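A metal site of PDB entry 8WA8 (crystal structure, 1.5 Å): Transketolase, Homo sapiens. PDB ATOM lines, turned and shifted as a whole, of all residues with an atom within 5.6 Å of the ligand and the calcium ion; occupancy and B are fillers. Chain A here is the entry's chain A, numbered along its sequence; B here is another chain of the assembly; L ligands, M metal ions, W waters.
The calcium ion is bound by the backbone carbonyl oxygen of Leu 187 (2.1 Å), the side-chain carboxylate of Asp 155 (2.1 Å), an oxygen (O2) of the ligand (2.1 Å), an oxygen (O7) of the ligand (2.2 Å), the side-chain amide oxygen of Asn 185 (2.2 Å) and water W3 (2.3 Å).
The calcium ion has six donor atoms within binding distance.
The side-chain amide oxygen (OE1) of Gln 189 sits close to a nitrogen (N4) of the ligand (3.4 Å).
Residues that only touch the ligand: Glu 160 (3.2 Å), Phe 392 of chain B (3.3 Å), Ile 364 of chain B (3.5 Å), Gly 154 (3.5 Å), Arg 395 of chain B (3.6 Å), Ser 124 (3.6 Å), Asp 341 of chain B (3.6 Å), Gln 428 of chain B (3.8 Å), Gly 188 (3.9 Å) and Thr 342 of chain B (3.95 Å).
Hydrophobic or aromatic side chains that line the ligand: His 77, Leu 125, His 258, Ile 364 of chain B and Phe 392 of chain B.
Of the 34 residues printed, 24 come within 4 Å of the ligand.
Water W3 lies within hydrogen-bond range of O6 of the ligand (2.7 Å), O of Asp 183 (2.7 Å), N of Asp 155 (3.0 Å) and ND2 of Asn 185 (3.2 Å).
Water W2 lies within hydrogen-bond range of N3 of the ligand (3.1 Å), OE1 of Gln 428 of chain B (3.3 Å) and O of Gly 123 (3.4 Å).
Water W1 lies within hydrogen-bond range of OG1 of Thr 388 of chain B (2.6 Å), OE2 of Glu 366 of chain B (2.8 Å) and O of Gly 340 of chain B (2.8 Å).
The guanidinium group (NH1) of Arg 395 of chain B lies within hydrogen-bond range of the side-chain hydroxyl (OG) of Ser 124 (3.1 Å).
OG of Ser 43 lies within hydrogen-bond range of ND2 of Asn 185, 3.0 Å away.
OD2 of Asp 155 is in hydrogen-bond range of N of Arg 186, at 2.9 Å.
The side-chain carboxylate (OE1) of Glu 366 of chain B sits close to the side-chain carboxylate (OE2) of Glu 160.
A ring nitrogen (ND1) of His 258 sits at hydrogen-bond distance from the side-chain amino group (NZ) of Lys 244 (2.8 Å).
NZ of Lys 244 sits at hydrogen-bond distance from O of Gly 188, 3.0 Å away.
The guanidinium group (NH1) of Arg 395 of chain B lies within salt-bridge range of the side-chain carboxylate (OD2) of Asp 398, at 2.9 Å.
The backbone carbonyl oxygen (O) of Ser 40 lies within hydrogen-bond range of the side-chain hydroxyl (OG) of Ser 43, 3.4 Å away.
The backbone carbonyl oxygen (O) of Gly 123 sits at hydrogen-bond distance from a nitrogen (N3) of the ligand.
An oxygen (O3) of the ligand lies within hydrogen-bond range of the backbone NH of Gly 156 (3.4 Å).
A nitrogen (N2) of the ligand sits at hydrogen-bond distance from the backbone NH (N) of Leu 125, 3.1 Å away.
OE2 of Glu 366 of chain B sits at hydrogen-bond distance from N1 of the ligand, at 2.7 Å.
O6 of the ligand is in salt-bridge range of NZ of Lys 75 (2.6 Å).
The backbone NH (N) of Glu 157 lies within hydrogen-bond range of an oxygen (O3) of the ligand (2.8 Å).
NZ of Lys 244 lies within salt-bridge range of O5 of the ligand (3.3 Å).
NE2 of His 77 is in hydrogen-bond range of O5 of the ligand, at 2.7 Å.
A ring nitrogen (NE2) of His 258 sits close to a sulfur (S1) of the ligand, at 3.4 Å.
O5 of the ligand is in hydrogen-bond range of OG of Ser 40 (2.5 Å).
Along chain A the residues within 4 Å of the calcium ion span positions 155 to 187.
The nearest printed residue that does not touch the calcium ion is Gly 156 (4.1 Å).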
ATOM      1  N   HIS A  37      23.607 -24.215  23.918  1.00  0.00           N
ATOM      2  CA  HIS A  37      22.965 -24.367  22.610  1.00  0.00           C
ATOM      3  C   HIS A  37      22.078 -25.608  22.570  1.00  0.00           C
ATOM      4  O   HIS A  37      22.297 -26.524  21.771  1.00  0.00           O
ATOM      5  CB  HIS A  37      24.030 -24.457  21.516  1.00  0.00           C
ATOM      6  CG  HIS A  37      24.919 -23.253  21.423  1.00  0.00           C
ATOM      7  ND1 HIS A  37      25.848 -22.927  22.390  1.00  0.00           N
ATOM      8  CD2 HIS A  37      25.023 -22.300  20.471  1.00  0.00           C
ATOM      9  CE1 HIS A  37      26.481 -21.819  22.038  1.00  0.00           C
ATOM     10  NE2 HIS A  37      26.006 -21.425  20.864  1.00  0.00           N
ATOM     11  N   SER A  40      20.789 -26.860  19.151  1.00  0.00           N
ATOM     12  CA  SER A  40      21.812 -27.496  18.323  1.00  0.00           C
ATOM     13  C   SER A  40      22.113 -28.912  18.786  1.00  0.00           C
ATOM     14  O   SER A  40      22.509 -29.760  17.971  1.00  0.00           O
ATOM     15  CB  SER A  40      23.111 -26.678  18.369  1.00  0.00           C
ATOM     16  OG  SER A  40      22.910 -25.346  17.931  1.00  0.00           O
ATOM     17  N   SER A  43      18.874 -31.314  17.475  1.00  0.00           N
ATOM     18  CA  SER A  43      18.815 -31.813  16.108  1.00  0.00           C
ATOM     19  C   SER A  43      19.681 -33.038  15.903  1.00  0.00           C
ATOM     20  O   SER A  43      19.437 -33.823  14.975  1.00  0.00           O
ATOM     21  CB  SER A  43      19.168 -30.710  15.099  1.00  0.00           C
ATOM     22  OG  SER A  43      20.468 -30.233  15.292  1.00  0.00           O
ATOM     23  N   LYS A  75      30.779 -29.582  15.063  1.00  0.00           N
ATOM     24  CA  LYS A  75      29.893 -28.515  15.553  1.00  0.00           C
ATOM     25  C   LYS A  75      29.989 -28.489  17.080  1.00  0.00           C
ATOM     26  O   LYS A  75      29.104 -28.963  17.808  1.00  0.00           O
ATOM     27  CB  LYS A  75      28.469 -28.666  15.033  1.00  0.00           C
ATOM     28  CG  LYS A  75      27.904 -30.086  15.054  1.00  0.00           C
ATOM     29  CD  LYS A  75      26.396 -30.099  14.675  1.00  0.00           C
ATOM     30  CE  LYS A  75      25.536 -29.849  15.908  1.00  0.00           C
ATOM     31  NZ  LYS A  75      24.085 -29.674  15.573  1.00  0.00           N
ATOM     32  N   HIS A  77      29.752 -26.455  19.535  1.00  0.00           N
ATOM     33  CA  HIS A  77      28.778 -25.856  20.447  1.00  0.00           C
ATOM     34  C   HIS A  77      27.691 -26.839  20.877  1.00  0.00           C
ATOM     35  O   HIS A  77      26.930 -26.520  21.796  1.00  0.00           O
ATOM     36  CB  HIS A  77      28.164 -24.604  19.820  1.00  0.00           C
ATOM     37  CG  HIS A  77      27.591 -24.842  18.455  1.00  0.00           C
ATOM     38  ND1 HIS A  77      28.379 -25.065  17.347  1.00  0.00           N
ATOM     39  CD2 HIS A  77      26.307 -24.905  18.036  1.00  0.00           C
ATOM     40  CE1 HIS A  77      27.599 -25.253  16.298  1.00  0.00           C
ATOM     41  NE2 HIS A  77      26.335 -25.160  16.685  1.00  0.00           N
ATOM     42  N   GLY A 123      35.007 -25.651  18.085  1.00  0.00           N
ATOM     43  CA  GLY A 123      34.437 -24.400  18.522  1.00  0.00           C
ATOM     44  C   GLY A 123      34.621 -23.371  17.429  1.00  0.00           C
ATOM     45  O   GLY A 123      33.757 -22.518  17.220  1.00  0.00           O
ATOM     46  N   SER A 124      35.744 -23.453  16.727  1.00  0.00           N
ATOM     47  CA  SER A 124      35.902 -22.719  15.473  1.00  0.00           C
ATOM     48  C   SER A 124      35.428 -23.645  14.364  1.00  0.00           C
ATOM     49  O   SER A 124      36.068 -24.670  14.087  1.00  0.00           O
ATOM     50  CB  SER A 124      37.360 -22.308  15.263  1.00  0.00           C
ATOM     51  OG  SER A 124      37.473 -21.683  14.001  1.00  0.00           O
ATOM     52  N   LEU A 125      34.293 -23.296  13.757  1.00  0.00           N
ATOM     53  CA  LEU A 125      33.605 -24.205  12.853  1.00  0.00           C
ATOM     54  C   LEU A 125      34.452 -24.507  11.611  1.00  0.00           C
ATOM     55  O   LEU A 125      35.244 -23.674  11.149  1.00  0.00           O
ATOM     56  CB  LEU A 125      32.284 -23.594  12.408  1.00  0.00           C
ATOM     57  CG  LEU A 125      31.244 -23.495  13.521  1.00  0.00           C
ATOM     58  CD1 LEU A 125      30.066 -22.643  13.058  1.00  0.00           C
ATOM     59  CD2 LEU A 125      30.770 -24.877  13.893  1.00  0.00           C
ATOM     60  N   GLY A 154      27.661 -29.319  11.307  1.00  0.00           N
ATOM     61  CA  GLY A 154      26.440 -28.579  11.064  1.00  0.00           C
ATOM     62  C   GLY A 154      26.314 -28.130   9.610  1.00  0.00           C
ATOM     63  O   GLY A 154      27.265 -28.221   8.818  1.00  0.00           O
ATOM     64  N   ASP A 155      25.139 -27.617   9.258  1.00  0.00           N
ATOM     65  CA  ASP A 155      24.971 -27.195   7.867  1.00  0.00           C
ATOM     66  C   ASP A 155      25.506 -25.785   7.608  1.00  0.00           C
ATOM     67  O   ASP A 155      26.115 -25.534   6.553  1.00  0.00           O
ATOM     68  CB  ASP A 155      23.533 -27.427   7.334  1.00  0.00           C
ATOM     69  CG  ASP A 155      22.437 -26.735   8.150  1.00  0.00           C
ATOM     70  OD1 ASP A 155      22.680 -26.213   9.241  1.00  0.00           O
ATOM     71  OD2 ASP A 155      21.283 -26.760   7.674  1.00  0.00           O
ATOM     72  N   GLY A 156      25.300 -24.858   8.548  1.00  0.00           N
ATOM     73  CA  GLY A 156      25.951 -23.561   8.421  1.00  0.00           C
ATOM     74  C   GLY A 156      27.459 -23.705   8.335  1.00  0.00           C
ATOM     75  O   GLY A 156      28.124 -23.026   7.541  1.00  0.00           O
ATOM     76  N   GLU A 157      28.008 -24.652   9.101  1.00  0.00           N
ATOM     77  CA  GLU A 157      29.438 -24.938   9.097  1.00  0.00           C
ATOM     78  C   GLU A 157      29.973 -25.295   7.712  1.00  0.00           C
ATOM     79  O   GLU A 157      31.150 -25.048   7.407  1.00  0.00           O
ATOM     80  CB  GLU A 157      29.668 -26.100  10.075  1.00  0.00           C
ATOM     81  CG  GLU A 157      31.069 -26.604  10.141  1.00  0.00           C
ATOM     82  CD  GLU A 157      31.293 -27.558  11.303  1.00  0.00           C
ATOM     83  OE1 GLU A 157      30.321 -28.203  11.789  1.00  0.00           O
ATOM     84  OE2 GLU A 157      32.455 -27.647  11.724  1.00  0.00           O
ATOM     85  N   LEU A 158      29.131 -25.884   6.855  1.00  0.00           N
ATOM     86  CA  LEU A 158      29.549 -26.296   5.513  1.00  0.00           C
ATOM     87  C   LEU A 158      29.857 -25.114   4.610  1.00  0.00           C
ATOM     88  O   LEU A 158      30.344 -25.330   3.489  1.00  0.00           O
ATOM     89  CB  LEU A 158      28.508 -27.208   4.865  1.00  0.00           C
ATOM     90  CG  LEU A 158      28.147 -28.411   5.740  1.00  0.00           C
ATOM     91  CD1 LEU A 158      27.027 -29.233   5.121  1.00  0.00           C
ATOM     92  CD2 LEU A 158      29.372 -29.285   6.015  1.00  0.00           C
ATOM     93  N   GLU A 160      32.231 -23.109   5.344  1.00  0.00           N
ATOM     94  CA  GLU A 160      33.665 -22.889   5.501  1.00  0.00           C
ATOM     95  C   GLU A 160      34.450 -23.647   4.435  1.00  0.00           C
ATOM     96  O   GLU A 160      34.288 -24.855   4.265  1.00  0.00           O
ATOM     97  CB  GLU A 160      34.152 -23.343   6.877  1.00  0.00           C
ATOM     98  CG  GLU A 160      33.720 -22.466   8.043  1.00  0.00           C
ATOM     99  CD  GLU A 160      34.440 -21.134   8.113  1.00  0.00           C
ATOM    100  OE1 GLU A 160      35.270 -20.804   7.238  1.00  0.00           O
ATOM    101  OE2 GLU A 160      34.187 -20.401   9.087  1.00  0.00           O
ATOM    102  N   ASP A 183      24.459 -32.528   9.812  1.00  0.00           N
ATOM    103  CA  ASP A 183      23.235 -32.226  10.550  1.00  0.00           C
ATOM    104  C   ASP A 183      22.535 -31.079   9.818  1.00  0.00           C
ATOM    105  O   ASP A 183      22.750 -29.904  10.114  1.00  0.00           O
ATOM    106  CB  ASP A 183      23.587 -31.894  11.993  1.00  0.00           C
ATOM    107  CG  ASP A 183      22.360 -31.624  12.876  1.00  0.00           C
ATOM    108  OD1 ASP A 183      21.221 -31.621  12.360  1.00  0.00           O
ATOM    109  OD2 ASP A 183      22.548 -31.427  14.104  1.00  0.00           O
ATOM    110  N   ASN A 185      19.916 -29.140   9.655  1.00  0.00           N
ATOM    111  CA  ASN A 185      18.764 -28.690  10.425  1.00  0.00           C
ATOM    112  C   ASN A 185      18.196 -27.356   9.944  1.00  0.00           C
ATOM    113  O   ASN A 185      17.398 -26.742  10.659  1.00  0.00           O
ATOM    114  CB  ASN A 185      19.058 -28.670  11.933  1.00  0.00           C
ATOM    115  CG  ASN A 185      20.123 -27.665  12.316  1.00  0.00           C
ATOM    116  OD1 ASN A 185      20.475 -26.771  11.537  1.00  0.00           O
ATOM    117  ND2 ASN A 185      20.660 -27.826  13.523  1.00  0.00           N
ATOM    118  N   ARG A 186      18.614 -26.912   8.758  1.00  0.00           N
ATOM    119  CA  ARG A 186      18.005 -25.803   8.006  1.00  0.00           C
ATOM    120  C   ARG A 186      18.507 -24.433   8.430  1.00  0.00           C
ATOM    121  O   ARG A 186      18.510 -23.493   7.617  1.00  0.00           O
ATOM    122  CB  ARG A 186      16.470 -25.860   8.032  1.00  0.00           C
ATOM    123  CG  ARG A 186      15.829 -25.021   6.940  1.00  0.00           C
ATOM    124  CD  ARG A 186      14.303 -25.097   6.974  1.00  0.00           C
ATOM    125  NE  ARG A 186      13.748 -24.497   8.187  1.00  0.00           N
ATOM    126  CZ  ARG A 186      13.538 -23.195   8.336  1.00  0.00           C
ATOM    127  NH1 ARG A 186      13.875 -22.313   7.402  1.00  0.00           N
ATOM    128  NH2 ARG A 186      12.965 -22.760   9.463  1.00  0.00           N
ATOM    129  N   LEU A 187      18.927 -24.281   9.688  1.00  0.00           N
ATOM    130  CA  LEU A 187      19.185 -22.975  10.269  1.00  0.00           C
ATOM    131  C   LEU A 187      20.626 -22.835  10.716  1.00  0.00           C
ATOM    132  O   LEU A 187      21.255 -23.799  11.177  1.00  0.00           O
ATOM    133  CB  LEU A 187      18.254 -22.736  11.482  1.00  0.00           C
ATOM    134  CG  LEU A 187      16.757 -22.739  11.165  1.00  0.00           C
ATOM    135  CD1 LEU A 187      15.927 -22.557  12.429  1.00  0.00           C
ATOM    136  CD2 LEU A 187      16.426 -21.656  10.139  1.00  0.00           C
ATOM    137  N   GLY A 188      21.152 -21.626  10.573  1.00  0.00           N
ATOM    138  CA  GLY A 188      22.407 -21.224  11.182  1.00  0.00           C
ATOM    139  C   GLY A 188      22.173 -20.464  12.473  1.00  0.00           C
ATOM    140  O   GLY A 188      21.192 -20.700  13.199  1.00  0.00           O
ATOM    141  N   GLN A 189      23.092 -19.537  12.768  1.00  0.00           N
ATOM    142  CA  GLN A 189      22.976 -18.750  13.988  1.00  0.00           C
ATOM    143  C   GLN A 189      21.951 -17.625  13.860  1.00  0.00           C
ATOM    144  O   GLN A 189      21.155 -17.393  14.789  1.00  0.00           O
ATOM    145  CB  GLN A 189      24.333 -18.155  14.366  1.00  0.00           C
ATOM    146  CG  GLN A 189      24.203 -17.092  15.459  1.00  0.00           C
ATOM    147  CD  GLN A 189      25.523 -16.699  16.063  1.00  0.00           C
ATOM    148  OE1 GLN A 189      26.441 -17.513  16.171  1.00  0.00           O
ATOM    149  NE2 GLN A 189      25.640 -15.439  16.476  1.00  0.00           N
ATOM    150  N   ALA A 193      20.438 -21.472   6.940  1.00  0.00           N
ATOM    151  CA  ALA A 193      21.622 -21.783   6.150  1.00  0.00           C
ATOM    152  C   ALA A 193      21.296 -21.627   4.667  1.00  0.00           C
ATOM    153  O   ALA A 193      20.142 -21.816   4.266  1.00  0.00           O
ATOM    154  CB  ALA A 193      22.100 -23.211   6.440  1.00  0.00           C
ATOM    155  N   LYS A 244      16.134 -28.171  13.755  1.00  0.00           N
ATOM    156  CA  LYS A 244      16.793 -27.564  14.899  1.00  0.00           C
ATOM    157  C   LYS A 244      15.789 -27.487  16.046  1.00  0.00           C
ATOM    158  O   LYS A 244      14.627 -27.141  15.840  1.00  0.00           O
ATOM    159  CB  LYS A 244      17.283 -26.167  14.531  1.00  0.00           C
ATOM    160  CG  LYS A 244      18.417 -25.662  15.394  1.00  0.00           C
ATOM    161  CD  LYS A 244      19.212 -24.551  14.690  1.00  0.00           C
ATOM    162  CE  LYS A 244      20.359 -24.048  15.559  1.00  0.00           C
ATOM    163  NZ  LYS A 244      21.363 -23.232  14.764  1.00  0.00           N
ATOM    164  N   HIS A 258      19.070 -19.927  18.349  1.00  0.00           N
ATOM    165  CA  HIS A 258      20.426 -20.445  18.370  1.00  0.00           C
ATOM    166  C   HIS A 258      21.175 -19.892  19.573  1.00  0.00           C
ATOM    167  O   HIS A 258      21.202 -18.686  19.792  1.00  0.00           O
ATOM    168  CB  HIS A 258      21.181 -20.043  17.097  1.00  0.00           C
ATOM    169  CG  HIS A 258      22.590 -20.552  17.077  1.00  0.00           C
ATOM    170  ND1 HIS A 258      22.918 -21.808  16.613  1.00  0.00           N
ATOM    171  CD2 HIS A 258      23.732 -19.993  17.529  1.00  0.00           C
ATOM    172  CE1 HIS A 258      24.224 -21.978  16.741  1.00  0.00           C
ATOM    173  NE2 HIS A 258      24.742 -20.895  17.299  1.00  0.00           N
ATOM    174  N   ASP A 398      43.919 -19.773  12.158  1.00  0.00           N
ATOM    175  CA  ASP A 398      42.859 -20.248  13.052  1.00  0.00           C
ATOM    176  C   ASP A 398      43.043 -21.730  13.375  1.00  0.00           C
ATOM    177  O   ASP A 398      42.800 -22.174  14.509  1.00  0.00           O
ATOM    178  CB  ASP A 398      41.491 -19.977  12.410  1.00  0.00           C
ATOM    179  CG  ASP A 398      40.317 -20.149  13.378  1.00  0.00           C
ATOM    180  OD1 ASP A 398      40.496 -20.097  14.611  1.00  0.00           O
ATOM    181  OD2 ASP A 398      39.180 -20.322  12.883  1.00  0.00           O
ATOM    182  N   GLY B 340      29.429 -12.434   9.073  1.00  0.00           N
ATOM    183  CA  GLY B 340      29.500 -13.863   8.840  1.00  0.00           C
ATOM    184  C   GLY B 340      28.582 -14.696   9.712  1.00  0.00           C
ATOM    185  O   GLY B 340      29.070 -15.469  10.550  1.00  0.00           O
ATOM    186  N   ASP B 341      27.270 -14.584   9.511  1.00  0.00           N
ATOM    187  CA  ASP B 341      26.270 -15.288  10.318  1.00  0.00           C
ATOM    188  C   ASP B 341      26.398 -14.987  11.807  1.00  0.00           C
ATOM    189  O   ASP B 341      26.032 -15.813  12.654  1.00  0.00           O
ATOM    190  CB  ASP B 341      26.254 -16.796  10.057  1.00  0.00           C
ATOM    191  CG  ASP B 341      25.013 -17.502  10.623  1.00  0.00           C
ATOM    192  OD1 ASP B 341      23.952 -16.849  10.741  1.00  0.00           O
ATOM    193  OD2 ASP B 341      25.109 -18.698  10.962  1.00  0.00           O
ATOM    194  N   THR B 342      26.910 -13.797  12.166  1.00  0.00           N
ATOM    195  CA  THR B 342      27.025 -13.425  13.572  1.00  0.00           C
ATOM    196  C   THR B 342      26.354 -12.088  13.885  1.00  0.00           C
ATOM    197  O   THR B 342      26.642 -11.497  14.924  1.00  0.00           O
ATOM    198  CB  THR B 342      28.488 -13.428  14.057  1.00  0.00           C
ATOM    199  OG1 THR B 342      29.299 -12.653  13.156  1.00  0.00           O
ATOM    200  CG2 THR B 342      29.041 -14.852  14.126  1.00  0.00           C
ATOM    201  N   ILE B 364      29.048 -18.382   7.133  1.00  0.00           N
ATOM    202  CA  ILE B 364      30.193 -18.779   7.949  1.00  0.00           C
ATOM    203  C   ILE B 364      31.388 -19.010   7.031  1.00  0.00           C
ATOM    204  O   ILE B 364      31.740 -20.151   6.706  1.00  0.00           O
ATOM    205  CB  ILE B 364      29.846 -19.996   8.824  1.00  0.00           C
ATOM    206  CG1 ILE B 364      28.562 -19.696   9.603  1.00  0.00           C
ATOM    207  CG2 ILE B 364      30.972 -20.277   9.819  1.00  0.00           C
ATOM    208  CD1 ILE B 364      28.048 -20.876  10.442  1.00  0.00           C
ATOM    209  N   GLU B 366      34.732 -16.597   6.706  1.00  0.00           N
ATOM    210  CA  GLU B 366      35.421 -15.353   7.029  1.00  0.00           C
ATOM    211  C   GLU B 366      36.440 -14.982   5.954  1.00  0.00           C
ATOM    212  O   GLU B 366      36.645 -13.795   5.679  1.00  0.00           O
ATOM    213  CB  GLU B 366      36.108 -15.472   8.382  1.00  0.00           C
ATOM    214  CG  GLU B 366      35.170 -15.661   9.563  1.00  0.00           C
ATOM    215  CD  GLU B 366      34.622 -17.067   9.703  1.00  0.00           C
ATOM    216  OE1 GLU B 366      35.160 -18.004   9.073  1.00  0.00           O
ATOM    217  OE2 GLU B 366      33.666 -17.239  10.464  1.00  0.00           O
ATOM    218  N   THR B 388      32.674  -9.937  12.670  1.00  0.00           N
ATOM    219  CA  THR B 388      32.484 -11.264  13.246  1.00  0.00           C
ATOM    220  C   THR B 388      33.112 -11.207  14.634  1.00  0.00           C
ATOM    221  O   THR B 388      33.522 -10.140  15.097  1.00  0.00           O
ATOM    222  CB  THR B 388      33.057 -12.369  12.355  1.00  0.00           C
ATOM    223  OG1 THR B 388      32.817 -13.648  12.953  1.00  0.00           O
ATOM    224  CG2 THR B 388      34.572 -12.206  12.159  1.00  0.00           C
ATOM    225  N   PHE B 389      33.206 -12.354  15.289  1.00  0.00           N
ATOM    226  CA  PHE B 389      34.012 -12.417  16.498  1.00  0.00           C
ATOM    227  C   PHE B 389      35.477 -12.201  16.124  1.00  0.00           C
ATOM    228  O   PHE B 389      35.971 -12.767  15.136  1.00  0.00           O
ATOM    229  CB  PHE B 389      33.902 -13.794  17.155  1.00  0.00           C
ATOM    230  CG  PHE B 389      32.567 -14.096  17.771  1.00  0.00           C
ATOM    231  CD1 PHE B 389      31.438 -13.378  17.442  1.00  0.00           C
ATOM    232  CD2 PHE B 389      32.463 -15.117  18.699  1.00  0.00           C
ATOM    233  CE1 PHE B 389      30.220 -13.667  18.017  1.00  0.00           C
ATOM    234  CE2 PHE B 389      31.241 -15.410  19.283  1.00  0.00           C
ATOM    235  CZ  PHE B 389      30.121 -14.683  18.938  1.00  0.00           C
ATOM    236  N   PHE B 392      37.657 -15.115  15.058  1.00  0.00           N
ATOM    237  CA  PHE B 392      37.494 -15.724  13.738  1.00  0.00           C
ATOM    238  C   PHE B 392      38.099 -14.904  12.619  1.00  0.00           C
ATOM    239  O   PHE B 392      38.188 -15.392  11.493  1.00  0.00           O
ATOM    240  CB  PHE B 392      36.016 -16.078  13.510  1.00  0.00           C
ATOM    241  CG  PHE B 392      35.466 -16.955  14.592  1.00  0.00           C
ATOM    242  CD1 PHE B 392      36.217 -18.024  15.077  1.00  0.00           C
ATOM    243  CD2 PHE B 392      34.233 -16.686  15.155  1.00  0.00           C
ATOM    244  CE1 PHE B 392      35.743 -18.817  16.096  1.00  0.00           C
ATOM    245  CE2 PHE B 392      33.751 -17.487  16.189  1.00  0.00           C
ATOM    246  CZ  PHE B 392      34.511 -18.547  16.659  1.00  0.00           C
ATOM    247  N   ARG B 395      40.976 -16.676  11.012  1.00  0.00           N
ATOM    248  CA  ARG B 395      40.677 -17.508   9.851  1.00  0.00           C
ATOM    249  C   ARG B 395      40.988 -16.793   8.533  1.00  0.00           C
ATOM    250  O   ARG B 395      41.215 -17.455   7.507  1.00  0.00           O
ATOM    251  CB  ARG B 395      39.203 -17.930   9.905  1.00  0.00           C
ATOM    252  CG  ARG B 395      38.816 -19.023   8.922  1.00  0.00           C
ATOM    253  CD  ARG B 395      39.499 -20.344   9.284  1.00  0.00           C
ATOM    254  NE  ARG B 395      38.703 -21.481   8.856  1.00  0.00           N
ATOM    255  CZ  ARG B 395      37.824 -22.114   9.617  1.00  0.00           C
ATOM    256  NH1 ARG B 395      37.612 -21.769  10.887  1.00  0.00           N
ATOM    257  NH2 ARG B 395      37.137 -23.122   9.106  1.00  0.00           N
ATOM    258  N   GLN B 428      36.242 -19.233  21.330  1.00  0.00           N
ATOM    259  CA  GLN B 428      35.569 -17.998  20.953  1.00  0.00           C
ATOM    260  C   GLN B 428      36.277 -16.752  21.466  1.00  0.00           C
ATOM    261  O   GLN B 428      35.822 -15.643  21.169  1.00  0.00           O
ATOM    262  CB  GLN B 428      34.117 -18.012  21.480  1.00  0.00           C
ATOM    263  CG  GLN B 428      33.414 -19.368  21.381  1.00  0.00           C
ATOM    264  CD  GLN B 428      33.140 -19.792  19.958  1.00  0.00           C
ATOM    265  OE1 GLN B 428      33.555 -20.873  19.537  1.00  0.00           O
ATOM    266  NE2 GLN B 428      32.431 -18.953  19.208  1.00  0.00           N
HETATM  267  N1  LIG L   1      32.820 -18.636  12.584  1.00  0.00           N
HETATM  268  C1  LIG L   1      33.518 -19.699  13.017  1.00  0.00           C
HETATM  269  C2  LIG L   1      34.712 -20.124  12.235  1.00  0.00           C
HETATM  270  N2  LIG L   1      33.219 -20.426  14.106  1.00  0.00           N
HETATM  271  C3  LIG L   1      32.155 -20.058  14.831  1.00  0.00           C
HETATM  272  N3  LIG L   1      31.892 -20.780  15.930  1.00  0.00           N
HETATM  273  C4  LIG L   1      31.344 -18.936  14.454  1.00  0.00           C
HETATM  274  C5  LIG L   1      31.747 -18.290  13.304  1.00  0.00           C
HETATM  275  C6  LIG L   1      30.136 -18.484  15.243  1.00  0.00           C
HETATM  276  N4  LIG L   1      29.100 -19.538  15.346  1.00  0.00           N
HETATM  277  C7  LIG L   1      29.051 -20.441  16.317  1.00  0.00           C
HETATM  278  S1  LIG L   1      27.805 -21.548  16.095  1.00  0.00           S
HETATM  279  C8  LIG L   1      27.329 -20.742  14.648  1.00  0.00           C
HETATM  280  C9  LIG L   1      28.139 -19.717  14.363  1.00  0.00           C
HETATM  281  C10 LIG L   1      28.064 -18.777  13.202  1.00  0.00           C
HETATM  282  C11 LIG L   1      26.206 -21.291  13.831  1.00  0.00           C
HETATM  283  C12 LIG L   1      26.392 -22.763  13.590  1.00  0.00           C
HETATM  284  O1  LIG L   1      25.443 -23.217  12.605  1.00  0.00           O
HETATM  285  P1  LIG L   1      25.396 -24.697  12.088  1.00  0.00           P
HETATM  286  O2  LIG L   1      24.285 -24.743  11.117  1.00  0.00           O
HETATM  287  O3  LIG L   1      26.777 -25.130  11.623  1.00  0.00           O
HETATM  288  O4  LIG L   1      25.049 -25.499  13.402  1.00  0.00           O
HETATM  289  P2  LIG L   1      23.762 -25.896  14.249  1.00  0.00           P
HETATM  290  O5  LIG L   1      23.875 -25.239  15.591  1.00  0.00           O
HETATM  291  O6  LIG L   1      23.788 -27.411  14.262  1.00  0.00           O
HETATM  292  O7  LIG L   1      22.602 -25.377  13.439  1.00  0.00           O
HETATM  293 CA    CA M   1      22.340 -25.643  11.283  1.00  0.00          CA
HETATM  294  O   HOH W   1      31.758 -15.407  11.345  1.00  0.00           O
HETATM  295  O   HOH W   2      30.622 -22.042  18.466  1.00  0.00           O
HETATM  296  O   HOH W   3      23.282 -27.705  11.647  1.00  0.00           O
